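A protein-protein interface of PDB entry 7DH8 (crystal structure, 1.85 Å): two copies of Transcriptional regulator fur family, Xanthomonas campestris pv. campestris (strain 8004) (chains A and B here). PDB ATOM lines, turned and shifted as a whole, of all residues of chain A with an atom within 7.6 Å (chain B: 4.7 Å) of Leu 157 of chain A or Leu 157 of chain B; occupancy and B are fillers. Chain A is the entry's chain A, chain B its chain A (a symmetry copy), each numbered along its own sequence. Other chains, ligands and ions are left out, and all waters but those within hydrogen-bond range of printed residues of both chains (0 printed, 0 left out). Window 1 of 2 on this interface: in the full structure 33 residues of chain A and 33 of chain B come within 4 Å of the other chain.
Pro 119 of chain A touches Leu 141 of chain B, and with the chains exchanged Leu 141 of chain A touches Pro 119 of chain B.
Val 137 of chain A touches Leu 141 of chain B, and with the chains exchanged Leu 141 of chain A touches Val 137 of chain B.
Thr 156 of chain B touches its own counterpart, Thr 156 of chain A.
Thr 156 of chain A touches Glu 158 of chain B, and with the chains exchanged Glu 158 of chain A touches Thr 156 of chain B.
Positions printed for both chains: 118, 119, 120, 137, 138, 141, 155, 156, 157, 158 and 159.
Of the 14 pairs that touch across the chains among the printed residues, 12 have their exchanged pair printed and touching as well.
N of Thr 156 of chain A sits at hydrogen-bond distance from O of Glu 158 of chain B (2.9 Å).
N of Thr 156 of chain B sits at hydrogen-bond distance from O of Glu 158 of chain A (2.9 Å).
A ring nitrogen (NE2) of His 160 of chain A lies within hydrogen-bond range of the side-chain hydroxyl of Thr 156 of chain B (2.9 Å).
O of Thr 156 of chain A sits close to O of Thr 156 of chain B (3.2 Å).
Asp 134 of chain A touches none of the printed residues of chain B.
Printed residues of chain B within 4 Å of Ala 154 of chain A: Val 159.
Leu 157 of chain A touches just these residues of chain B: Thr 156 (3.4 Å) and Leu 157 (3.8 Å).
Of the printed residues of chain B, Glu 158 of chain A touches Gln 155 and Thr 156.
Printed residues of chain A within 4 Å of Pro 119 of chain B: Leu 141.
Val 138 of chain B touches none of the printed residues of chain A.
Printed residues of chain A within 4 Å of Leu 141 of chain B: Pro 119 (3.7 Å) and Val 137 (3.99 Å).
Of chain A, only Thr 156 and Leu 157 come within 4 Å of Leu 157 of chain B.
The nearest residue of chain A that does not touch Leu 157 of chain B is Leu 141 of chain A (4.9 Å).
The nearest printed residue of chain B that does not touch Ala 154 of chain A is Glu 158 of chain B (4.3 Å).
CD2 of Leu 141 of chain B touches CG of Pro 119 of chain A, 3.7 Å away.
Val 137 of chain A touches Leu 141 of chain B (CG2 to CD2, 3.99 Å).
Leu 141 of chain A touches Pro 119 of chain B.
Val 137 of chain B touches Leu 141 of chain A (CG2 to CD2, 3.99 Å).
Val 159 of chain B touches Ala 154 of chain A.
Gln 155 of chain A touches Glu 158 of chain B.
CA of Leu 157 of chain B touches O of Thr 156 of chain A (3.4 Å).
Leu 157 of chain A touches Thr 156 of chain B.
Leu 157 of chain B touches Leu 157 of chain A (CD2 to CD2, 3.8 Å).
Glu 158 of chain A touches Gln 155 of chain B (O to CA, 3.6 Å).
The backbone NH (N) of Gln 155 of chain A lies within hydrogen-bond range of the side-chain hydroxyl (OG) of Ser 117 of chain A (2.9 Å).
The backbone NH (N) of Phe 120 of chain A is in hydrogen-bond range of the backbone carbonyl oxygen (O) of Leu 157 of chain A (3.0 Å).
NE2 of Gln 155 of chain A sits at hydrogen-bond distance from O of Val 138 of chain A (3.0 Å).
The backbone carbonyl oxygen (O) of Leu 157 of chain B lies within hydrogen-bond range of the backbone NH (N) of Phe 120 of chain B.
The backbone carbonyl oxygen (O) of Phe 120 of chain B sits at hydrogen-bond distance from the backbone NH (N) of Val 159 of chain B, 2.6 Å away.
O of Val 138 of chain B lies within hydrogen-bond range of NE2 of Gln 155 of chain B (3.0 Å).
Of the 21 printed residues of chain A, 9 touch a printed residue of chain B.
Printed residues of chain A that touch a printed residue of chain B: Pro 119, Val 137, Leu 141, Ala 154, Gln 155, Thr 156, Leu 157, Glu 158 and His 160.
Hydrophobic or aromatic side chains of chain A that line the printed part of chain B: Pro 119, Val 137, Leu 141, Leu 157 and His 160.
Of the 11 printed residues of chain B, 8 touch a printed residue of chain A.
Hydrophobic or aromatic side chains of chain B within 4 Å of the printed part of chain A: Pro 119, Val 137, Leu 141 and Leu 157.
Among the printed residues, 14 pairs touch across the chains.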
ATOM      1  N   LEU A  99      27.877  -5.020 -31.943  1.00  0.00           N
ATOM      2  CA  LEU A  99      26.730  -4.118 -31.778  1.00  0.00           C
ATOM      3  C   LEU A  99      26.479  -3.405 -33.099  1.00  0.00           C
ATOM      4  O   LEU A  99      27.268  -2.560 -33.512  1.00  0.00           O
ATOM      5  CB  LEU A  99      27.019  -3.112 -30.680  1.00  0.00           C
ATOM      6  CG  LEU A  99      27.256  -3.848 -29.344  1.00  0.00           C
ATOM      7  CD1 LEU A  99      27.649  -2.858 -28.257  1.00  0.00           C
ATOM      8  CD2 LEU A  99      25.998  -4.721 -28.943  1.00  0.00           C
ATOM      9  N   GLU A 100      25.354  -3.710 -33.741  1.00  0.00           N
ATOM     10  CA  GLU A 100      25.148  -3.191 -35.083  1.00  0.00           C
ATOM     11  C   GLU A 100      24.904  -1.710 -35.116  1.00  0.00           C
ATOM     12  O   GLU A 100      25.250  -1.074 -36.115  1.00  0.00           O
ATOM     13  CB  GLU A 100      23.975  -3.899 -35.759  1.00  0.00           C
ATOM     14  CG  GLU A 100      24.150  -5.359 -35.763  1.00  0.00           C
ATOM     15  CD  GLU A 100      25.032  -5.812 -36.907  1.00  0.00           C
ATOM     16  OE1 GLU A 100      25.321  -4.975 -37.772  1.00  0.00           O
ATOM     17  OE2 GLU A 100      25.430  -7.002 -36.931  1.00  0.00           O
ATOM     18  N   SER A 101      24.285  -1.125 -34.075  1.00  0.00           N
ATOM     19  CA  SER A 101      23.976   0.295 -34.223  1.00  0.00           C
ATOM     20  C   SER A 101      25.166   1.214 -33.949  1.00  0.00           C
ATOM     21  O   SER A 101      25.083   2.415 -34.266  1.00  0.00           O
ATOM     22  CB  SER A 101      22.798   0.707 -33.319  1.00  0.00           C
ATOM     23  OG  SER A 101      23.133   0.548 -31.969  1.00  0.00           O
ATOM     24  N   SER A 117      20.901 -14.659 -28.766  1.00  0.00           N
ATOM     25  CA  SER A 117      20.371 -13.339 -29.049  1.00  0.00           C
ATOM     26  C   SER A 117      19.945 -12.734 -27.723  1.00  0.00           C
ATOM     27  O   SER A 117      19.288 -13.420 -26.916  1.00  0.00           O
ATOM     28  CB  SER A 117      19.198 -13.455 -30.029  1.00  0.00           C
ATOM     29  OG  SER A 117      19.795 -13.786 -31.278  1.00  0.00           O
ATOM     30  N   VAL A 118      20.383 -11.491 -27.471  1.00  0.00           N
ATOM     31  CA  VAL A 118      20.103 -10.826 -26.188  1.00  0.00           C
ATOM     32  C   VAL A 118      19.992  -9.324 -26.403  1.00  0.00           C
ATOM     33  O   VAL A 118      20.665  -8.778 -27.265  1.00  0.00           O
ATOM     34  CB  VAL A 118      21.187 -11.081 -25.129  1.00  0.00           C
ATOM     35  CG1 VAL A 118      21.172 -12.509 -24.655  1.00  0.00           C
ATOM     36  CG2 VAL A 118      22.580 -10.594 -25.645  1.00  0.00           C
ATOM     37  N   PRO A 119      19.185  -8.638 -25.617  1.00  0.00           N
ATOM     38  CA  PRO A 119      19.169  -7.175 -25.653  1.00  0.00           C
ATOM     39  C   PRO A 119      20.441  -6.587 -25.063  1.00  0.00           C
ATOM     40  O   PRO A 119      21.031  -7.108 -24.106  1.00  0.00           O
ATOM     41  CB  PRO A 119      17.958  -6.813 -24.768  1.00  0.00           C
ATOM     42  CG  PRO A 119      17.145  -8.134 -24.669  1.00  0.00           C
ATOM     43  CD  PRO A 119      18.197  -9.184 -24.679  1.00  0.00           C
ATOM     44  N   PHE A 120      20.773  -5.439 -25.594  1.00  0.00           N
ATOM     45  CA  PHE A 120      21.788  -4.523 -25.109  1.00  0.00           C
ATOM     46  C   PHE A 120      21.162  -3.173 -24.858  1.00  0.00           C
ATOM     47  O   PHE A 120      20.378  -2.702 -25.694  1.00  0.00           O
ATOM     48  CB  PHE A 120      22.905  -4.346 -26.174  1.00  0.00           C
ATOM     49  CG  PHE A 120      23.747  -5.533 -26.296  1.00  0.00           C
ATOM     50  CD1 PHE A 120      23.395  -6.537 -27.180  1.00  0.00           C
ATOM     51  CD2 PHE A 120      24.861  -5.690 -25.503  1.00  0.00           C
ATOM     52  CE1 PHE A 120      24.138  -7.683 -27.257  1.00  0.00           C
ATOM     53  CE2 PHE A 120      25.606  -6.850 -25.587  1.00  0.00           C
ATOM     54  CZ  PHE A 120      25.250  -7.826 -26.455  1.00  0.00           C
ATOM     55  N   LEU A 121      21.518  -2.546 -23.707  1.00  0.00           N
ATOM     56  CA  LEU A 121      21.218  -1.148 -23.436  1.00  0.00           C
ATOM     57  C   LEU A 121      22.458  -0.353 -23.817  1.00  0.00           C
ATOM     58  O   LEU A 121      23.524  -0.569 -23.244  1.00  0.00           O
ATOM     59  CB  LEU A 121      20.900  -0.921 -21.954  1.00  0.00           C
ATOM     60  CG  LEU A 121      19.845  -1.857 -21.322  1.00  0.00           C
ATOM     61  CD1 LEU A 121      19.725  -1.630 -19.851  1.00  0.00           C
ATOM     62  CD2 LEU A 121      18.501  -1.695 -22.082  1.00  0.00           C
ATOM     63  N   ILE A 122      22.337   0.553 -24.769  1.00  0.00           N
ATOM     64  CA  ILE A 122      23.495   1.282 -25.267  1.00  0.00           C
ATOM     65  C   ILE A 122      23.246   2.752 -25.026  1.00  0.00           C
ATOM     66  O   ILE A 122      22.276   3.307 -25.526  1.00  0.00           O
ATOM     67  CB  ILE A 122      23.764   0.981 -26.754  1.00  0.00           C
ATOM     68  CG1 ILE A 122      23.977  -0.505 -26.959  1.00  0.00           C
ATOM     69  CG2 ILE A 122      25.069   1.724 -27.259  1.00  0.00           C
ATOM     70  CD1 ILE A 122      23.995  -0.874 -28.533  1.00  0.00           C
ATOM     71  N   VAL A 130      25.250  -2.441 -22.046  1.00  0.00           N
ATOM     72  CA  VAL A 130      24.970  -3.443 -21.020  1.00  0.00           C
ATOM     73  C   VAL A 130      24.232  -4.583 -21.696  1.00  0.00           C
ATOM     74  O   VAL A 130      23.202  -4.357 -22.345  1.00  0.00           O
ATOM     75  CB  VAL A 130      24.134  -2.875 -19.866  1.00  0.00           C
ATOM     76  CG1 VAL A 130      23.807  -4.028 -18.851  1.00  0.00           C
ATOM     77  CG2 VAL A 130      24.890  -1.755 -19.150  1.00  0.00           C
ATOM     78  N   ASP A 134      16.958 -11.931 -22.063  1.00  0.00           N
ATOM     79  CA  ASP A 134      15.484 -12.055 -21.976  1.00  0.00           C
ATOM     80  C   ASP A 134      15.119 -13.171 -22.958  1.00  0.00           C
ATOM     81  O   ASP A 134      15.295 -13.008 -24.166  1.00  0.00           O
ATOM     82  CB  ASP A 134      14.943 -10.685 -22.333  1.00  0.00           C
ATOM     83  CG  ASP A 134      13.545 -10.458 -21.741  1.00  0.00           C
ATOM     84  OD1 ASP A 134      12.649 -11.308 -21.955  1.00  0.00           O
ATOM     85  OD2 ASP A 134      13.365  -9.452 -21.000  1.00  0.00           O
ATOM     86  N   VAL A 137      11.364 -12.073 -24.479  1.00  0.00           N
ATOM     87  CA  VAL A 137      11.397 -11.157 -25.627  1.00  0.00           C
ATOM     88  C   VAL A 137      11.842 -11.879 -26.882  1.00  0.00           C
ATOM     89  O   VAL A 137      11.253 -11.686 -27.961  1.00  0.00           O
ATOM     90  CB  VAL A 137      12.297  -9.944 -25.341  1.00  0.00           C
ATOM     91  CG1 VAL A 137      12.674  -9.215 -26.678  1.00  0.00           C
ATOM     92  CG2 VAL A 137      11.588  -8.977 -24.390  1.00  0.00           C
ATOM     93  N   VAL A 138      12.906 -12.696 -26.781  1.00  0.00           N
ATOM     94  CA  VAL A 138      13.431 -13.345 -27.987  1.00  0.00           C
ATOM     95  C   VAL A 138      12.415 -14.371 -28.507  1.00  0.00           C
ATOM     96  O   VAL A 138      12.154 -14.446 -29.716  1.00  0.00           O
ATOM     97  CB  VAL A 138      14.806 -13.963 -27.663  1.00  0.00           C
ATOM     98  CG1 VAL A 138      15.194 -15.158 -28.619  1.00  0.00           C
ATOM     99  CG2 VAL A 138      15.859 -12.869 -27.607  1.00  0.00           C
ATOM    100  N   LEU A 141       9.465 -12.612 -30.333  1.00  0.00           N
ATOM    101  CA  LEU A 141       9.809 -12.202 -31.688  1.00  0.00           C
ATOM    102  C   LEU A 141       9.990 -13.392 -32.611  1.00  0.00           C
ATOM    103  O   LEU A 141       9.666 -13.304 -33.808  1.00  0.00           O
ATOM    104  CB  LEU A 141      11.085 -11.348 -31.662  1.00  0.00           C
ATOM    105  CG  LEU A 141      10.940  -9.916 -31.142  1.00  0.00           C
ATOM    106  CD1 LEU A 141      12.376  -9.186 -31.156  1.00  0.00           C
ATOM    107  CD2 LEU A 141       9.918  -9.162 -31.964  1.00  0.00           C
ATOM    108  N   ALA A 154      18.952 -15.037 -35.708  1.00  0.00           N
ATOM    109  CA  ALA A 154      19.810 -14.318 -34.765  1.00  0.00           C
ATOM    110  C   ALA A 154      18.976 -13.032 -34.793  1.00  0.00           C
ATOM    111  O   ALA A 154      18.534 -12.557 -35.848  1.00  0.00           O
ATOM    112  CB  ALA A 154      21.206 -13.801 -35.150  1.00  0.00           C
ATOM    113  N   GLN A 155      18.786 -12.438 -33.604  1.00  0.00           N
ATOM    114  CA  GLN A 155      18.147 -11.138 -33.465  1.00  0.00           C
ATOM    115  C   GLN A 155      19.069 -10.036 -32.978  1.00  0.00           C
ATOM    116  O   GLN A 155      19.832 -10.247 -32.032  1.00  0.00           O
ATOM    117  CB  GLN A 155      16.994 -11.285 -32.428  1.00  0.00           C
ATOM    118  CG  GLN A 155      16.007 -12.422 -32.823  1.00  0.00           C
ATOM    119  CD  GLN A 155      14.863 -12.521 -31.806  1.00  0.00           C
ATOM    120  OE1 GLN A 155      14.668 -11.609 -31.011  1.00  0.00           O
ATOM    121  NE2 GLN A 155      14.124 -13.620 -31.825  1.00  0.00           N
ATOM    122  N   THR A 156      18.905  -8.828 -33.544  1.00  0.00           N
ATOM    123  CA  THR A 156      19.628  -7.642 -33.121  1.00  0.00           C
ATOM    124  C   THR A 156      18.661  -6.838 -32.287  1.00  0.00           C
ATOM    125  O   THR A 156      17.640  -6.379 -32.814  1.00  0.00           O
ATOM    126  CB  THR A 156      20.072  -6.804 -34.331  1.00  0.00           C
ATOM    127  OG1 THR A 156      21.003  -7.552 -35.092  1.00  0.00           O
ATOM    128  CG2 THR A 156      20.758  -5.505 -33.833  1.00  0.00           C
ATOM    129  N   LEU A 157      18.960  -6.692 -30.987  1.00  0.00           N
ATOM    130  CA  LEU A 157      18.078  -6.047 -30.029  1.00  0.00           C
ATOM    131  C   LEU A 157      18.949  -5.030 -29.296  1.00  0.00           C
ATOM    132  O   LEU A 157      19.792  -5.365 -28.457  1.00  0.00           O
ATOM    133  CB  LEU A 157      17.424  -7.042 -29.053  1.00  0.00           C
ATOM    134  CG  LEU A 157      16.831  -8.292 -29.768  1.00  0.00           C
ATOM    135  CD1 LEU A 157      16.676  -9.375 -28.704  1.00  0.00           C
ATOM    136  CD2 LEU A 157      15.517  -7.927 -30.437  1.00  0.00           C
ATOM    137  N   GLU A 158      18.770  -3.768 -29.617  1.00  0.00           N
ATOM    138  CA  GLU A 158      19.622  -2.755 -28.997  1.00  0.00           C
ATOM    139  C   GLU A 158      18.730  -1.616 -28.535  1.00  0.00           C
ATOM    140  O   GLU A 158      18.082  -0.957 -29.342  1.00  0.00           O
ATOM    141  CB  GLU A 158      20.685  -2.312 -29.985  1.00  0.00           C
ATOM    142  CG  GLU A 158      21.528  -3.527 -30.494  1.00  0.00           C
ATOM    143  CD  GLU A 158      22.627  -3.186 -31.537  1.00  0.00           C
ATOM    144  OE1 GLU A 158      22.702  -2.059 -32.031  1.00  0.00           O
ATOM    145  OE2 GLU A 158      23.405  -4.098 -31.864  1.00  0.00           O
ATOM    146  N   VAL A 159      18.722  -1.356 -27.254  1.00  0.00           N
ATOM    147  CA  VAL A 159      17.870  -0.308 -26.708  1.00  0.00           C
ATOM    148  C   VAL A 159      18.717   0.941 -26.565  1.00  0.00           C
ATOM    149  O   VAL A 159      19.763   0.906 -25.893  1.00  0.00           O
ATOM    150  CB  VAL A 159      17.254  -0.757 -25.375  1.00  0.00           C
ATOM    151  CG1 VAL A 159      16.424   0.366 -24.766  1.00  0.00           C
ATOM    152  CG2 VAL A 159      16.392  -2.007 -25.619  1.00  0.00           C
ATOM    153  N   HIS A 160      18.243   2.058 -27.136  1.00  0.00           N
ATOM    154  CA  HIS A 160      18.946   3.333 -27.028  1.00  0.00           C
ATOM    155  C   HIS A 160      18.304   4.265 -26.003  1.00  0.00           C
ATOM    156  O   HIS A 160      17.151   4.104 -25.597  1.00  0.00           O
ATOM    157  CB  HIS A 160      19.001   4.049 -28.377  1.00  0.00           C
ATOM    158  CG  HIS A 160      19.385   3.143 -29.503  1.00  0.00           C
ATOM    159  ND1 HIS A 160      20.703   2.813 -29.787  1.00  0.00           N
ATOM    160  CD2 HIS A 160      18.617   2.503 -30.429  1.00  0.00           C
ATOM    161  CE1 HIS A 160      20.726   1.999 -30.838  1.00  0.00           C
ATOM    162  NE2 HIS A 160      19.473   1.777 -31.227  1.00  0.00           N
ATOM    163  N   VAL B 118       9.792  -0.525 -33.736  1.00  0.00           N
ATOM    164  CA  VAL B 118       9.064  -1.709 -34.221  1.00  0.00           C
ATOM    165  C   VAL B 118      10.055  -2.758 -34.702  1.00  0.00           C
ATOM    166  O   VAL B 118      11.113  -2.415 -35.208  1.00  0.00           O
ATOM    167  CB  VAL B 118       8.103  -1.390 -35.376  1.00  0.00           C
ATOM    168  CG1 VAL B 118       6.928  -0.574 -34.910  1.00  0.00           C
ATOM    169  CG2 VAL B 118       8.881  -0.761 -36.577  1.00  0.00           C
ATOM    170  N   PRO B 119       9.723  -4.029 -34.587  1.00  0.00           N
ATOM    171  CA  PRO B 119      10.548  -5.077 -35.191  1.00  0.00           C
ATOM    172  C   PRO B 119      10.449  -5.062 -36.708  1.00  0.00           C
ATOM    173  O   PRO B 119       9.398  -4.778 -37.301  1.00  0.00           O
ATOM    174  CB  PRO B 119       9.934  -6.377 -34.632  1.00  0.00           C
ATOM    175  CG  PRO B 119       9.085  -5.911 -33.417  1.00  0.00           C
ATOM    176  CD  PRO B 119       8.583  -4.578 -33.842  1.00  0.00           C
ATOM    177  N   PHE B 120      11.538  -5.480 -37.300  1.00  0.00           N
ATOM    178  CA  PHE B 120      11.690  -5.797 -38.707  1.00  0.00           C
ATOM    179  C   PHE B 120      12.177  -7.218 -38.850  1.00  0.00           C
ATOM    180  O   PHE B 120      13.087  -7.623 -38.113  1.00  0.00           O
ATOM    181  CB  PHE B 120      12.743  -4.857 -39.359  1.00  0.00           C
ATOM    182  CG  PHE B 120      12.248  -3.492 -39.511  1.00  0.00           C
ATOM    183  CD1 PHE B 120      12.421  -2.580 -38.485  1.00  0.00           C
ATOM    184  CD2 PHE B 120      11.564  -3.114 -40.645  1.00  0.00           C
ATOM    185  CE1 PHE B 120      11.905  -1.317 -38.589  1.00  0.00           C
ATOM    186  CE2 PHE B 120      11.046  -1.837 -40.741  1.00  0.00           C
ATOM    187  CZ  PHE B 120      11.221  -0.954 -39.729  1.00  0.00           C
ATOM    188  N   VAL B 137       6.445  -6.301 -26.948  1.00  0.00           N
ATOM    189  CA  VAL B 137       7.906  -6.448 -26.981  1.00  0.00           C
ATOM    190  C   VAL B 137       8.590  -5.146 -26.619  1.00  0.00           C
ATOM    191  O   VAL B 137       9.563  -5.142 -25.844  1.00  0.00           O
ATOM    192  CB  VAL B 137       8.378  -6.956 -28.353  1.00  0.00           C
ATOM    193  CG1 VAL B 137       9.917  -6.700 -28.530  1.00  0.00           C
ATOM    194  CG2 VAL B 137       8.068  -8.447 -28.498  1.00  0.00           C
ATOM    195  N   VAL B 138       8.123  -4.022 -27.192  1.00  0.00           N
ATOM    196  CA  VAL B 138       8.810  -2.750 -26.944  1.00  0.00           C
ATOM    197  C   VAL B 138       8.627  -2.341 -25.477  1.00  0.00           C
ATOM    198  O   VAL B 138       9.583  -1.908 -24.817  1.00  0.00           O
ATOM    199  CB  VAL B 138       8.283  -1.696 -27.939  1.00  0.00           C
ATOM    200  CG1 VAL B 138       8.455  -0.213 -27.426  1.00  0.00           C
ATOM    201  CG2 VAL B 138       8.893  -1.935 -29.310  1.00  0.00           C
ATOM    202  N   LEU B 141      10.939  -4.427 -23.147  1.00  0.00           N
ATOM    203  CA  LEU B 141      12.317  -3.952 -23.153  1.00  0.00           C
ATOM    204  C   LEU B 141      12.453  -2.599 -22.480  1.00  0.00           C
ATOM    205  O   LEU B 141      13.484  -2.323 -21.842  1.00  0.00           O
ATOM    206  CB  LEU B 141      12.835  -3.884 -24.597  1.00  0.00           C
ATOM    207  CG  LEU B 141      13.170  -5.219 -25.268  1.00  0.00           C
ATOM    208  CD1 LEU B 141      13.663  -4.957 -26.780  1.00  0.00           C
ATOM    209  CD2 LEU B 141      14.208  -5.964 -24.459  1.00  0.00           C
ATOM    210  N   GLN B 155      14.317   1.927 -29.917  1.00  0.00           N
ATOM    211  CA  GLN B 155      14.872   0.583 -29.989  1.00  0.00           C
ATOM    212  C   GLN B 155      15.117   0.081 -31.399  1.00  0.00           C
ATOM    213  O   GLN B 155      14.255   0.241 -32.266  1.00  0.00           O
ATOM    214  CB  GLN B 155      13.856  -0.385 -29.311  1.00  0.00           C
ATOM    215  CG  GLN B 155      13.510   0.067 -27.862  1.00  0.00           C
ATOM    216  CD  GLN B 155      12.538  -0.922 -27.207  1.00  0.00           C
ATOM    217  OE1 GLN B 155      12.358  -2.027 -27.704  1.00  0.00           O
ATOM    218  NE2 GLN B 155      11.912  -0.524 -26.108  1.00  0.00           N
ATOM    219  N   THR B 156      16.238  -0.635 -31.590  1.00  0.00           N
ATOM    220  CA  THR B 156      16.572  -1.278 -32.848  1.00  0.00           C
ATOM    221  C   THR B 156      16.255  -2.742 -32.668  1.00  0.00           C
ATOM    222  O   THR B 156      16.886  -3.401 -31.832  1.00  0.00           O
ATOM    223  CB  THR B 156      18.066  -1.119 -33.172  1.00  0.00           C
ATOM    224  OG1 THR B 156      18.351   0.254 -33.372  1.00  0.00           O
ATOM    225  CG2 THR B 156      18.397  -1.896 -34.473  1.00  0.00           C
ATOM    226  N   LEU B 157      15.264  -3.244 -33.420  1.00  0.00           N
ATOM    227  CA  LEU B 157      14.760  -4.600 -33.283  1.00  0.00           C
ATOM    228  C   LEU B 157      14.752  -5.174 -34.698  1.00  0.00           C
ATOM    229  O   LEU B 157      13.917  -4.835 -35.542  1.00  0.00           O
ATOM    230  CB  LEU B 157      13.365  -4.660 -32.638  1.00  0.00           C
ATOM    231  CG  LEU B 157      13.248  -3.774 -31.362  1.00  0.00           C
ATOM    232  CD1 LEU B 157      11.760  -3.536 -31.126  1.00  0.00           C
ATOM    233  CD2 LEU B 157      13.930  -4.464 -30.192  1.00  0.00           C
ATOM    234  N   GLU B 158      15.696  -6.042 -34.982  1.00  0.00           N
ATOM    235  CA  GLU B 158      15.779  -6.576 -36.341  1.00  0.00           C
ATOM    236  C   GLU B 158      15.959  -8.080 -36.240  1.00  0.00           C
ATOM    237  O   GLU B 158      16.956  -8.560 -35.709  1.00  0.00           O
ATOM    238  CB  GLU B 158      16.908  -5.891 -37.087  1.00  0.00           C
ATOM    239  CG  GLU B 158      16.723  -4.339 -37.098  1.00  0.00           C
ATOM    240  CD  GLU B 158      17.846  -3.538 -37.812  1.00  0.00           C
ATOM    241  OE1 GLU B 158      18.877  -4.096 -38.192  1.00  0.00           O
ATOM    242  OE2 GLU B 158      17.669  -2.317 -37.959  1.00  0.00           O
ATOM    243  N   VAL B 159      15.028  -8.823 -36.779  1.00  0.00           N
ATOM    244  CA  VAL B 159      15.092 -10.276 -36.701  1.00  0.00           C
ATOM    245  C   VAL B 159      15.702 -10.777 -37.996  1.00  0.00           C
ATOM    246  O   VAL B 159      15.181 -10.472 -39.084  1.00  0.00           O
ATOM    247  CB  VAL B 159      13.695 -10.861 -36.444  1.00  0.00           C
ATOM    248  CG1 VAL B 159      13.749 -12.384 -36.438  1.00  0.00           C
ATOM    249  CG2 VAL B 159      13.169 -10.325 -35.102  1.00  0.00           C
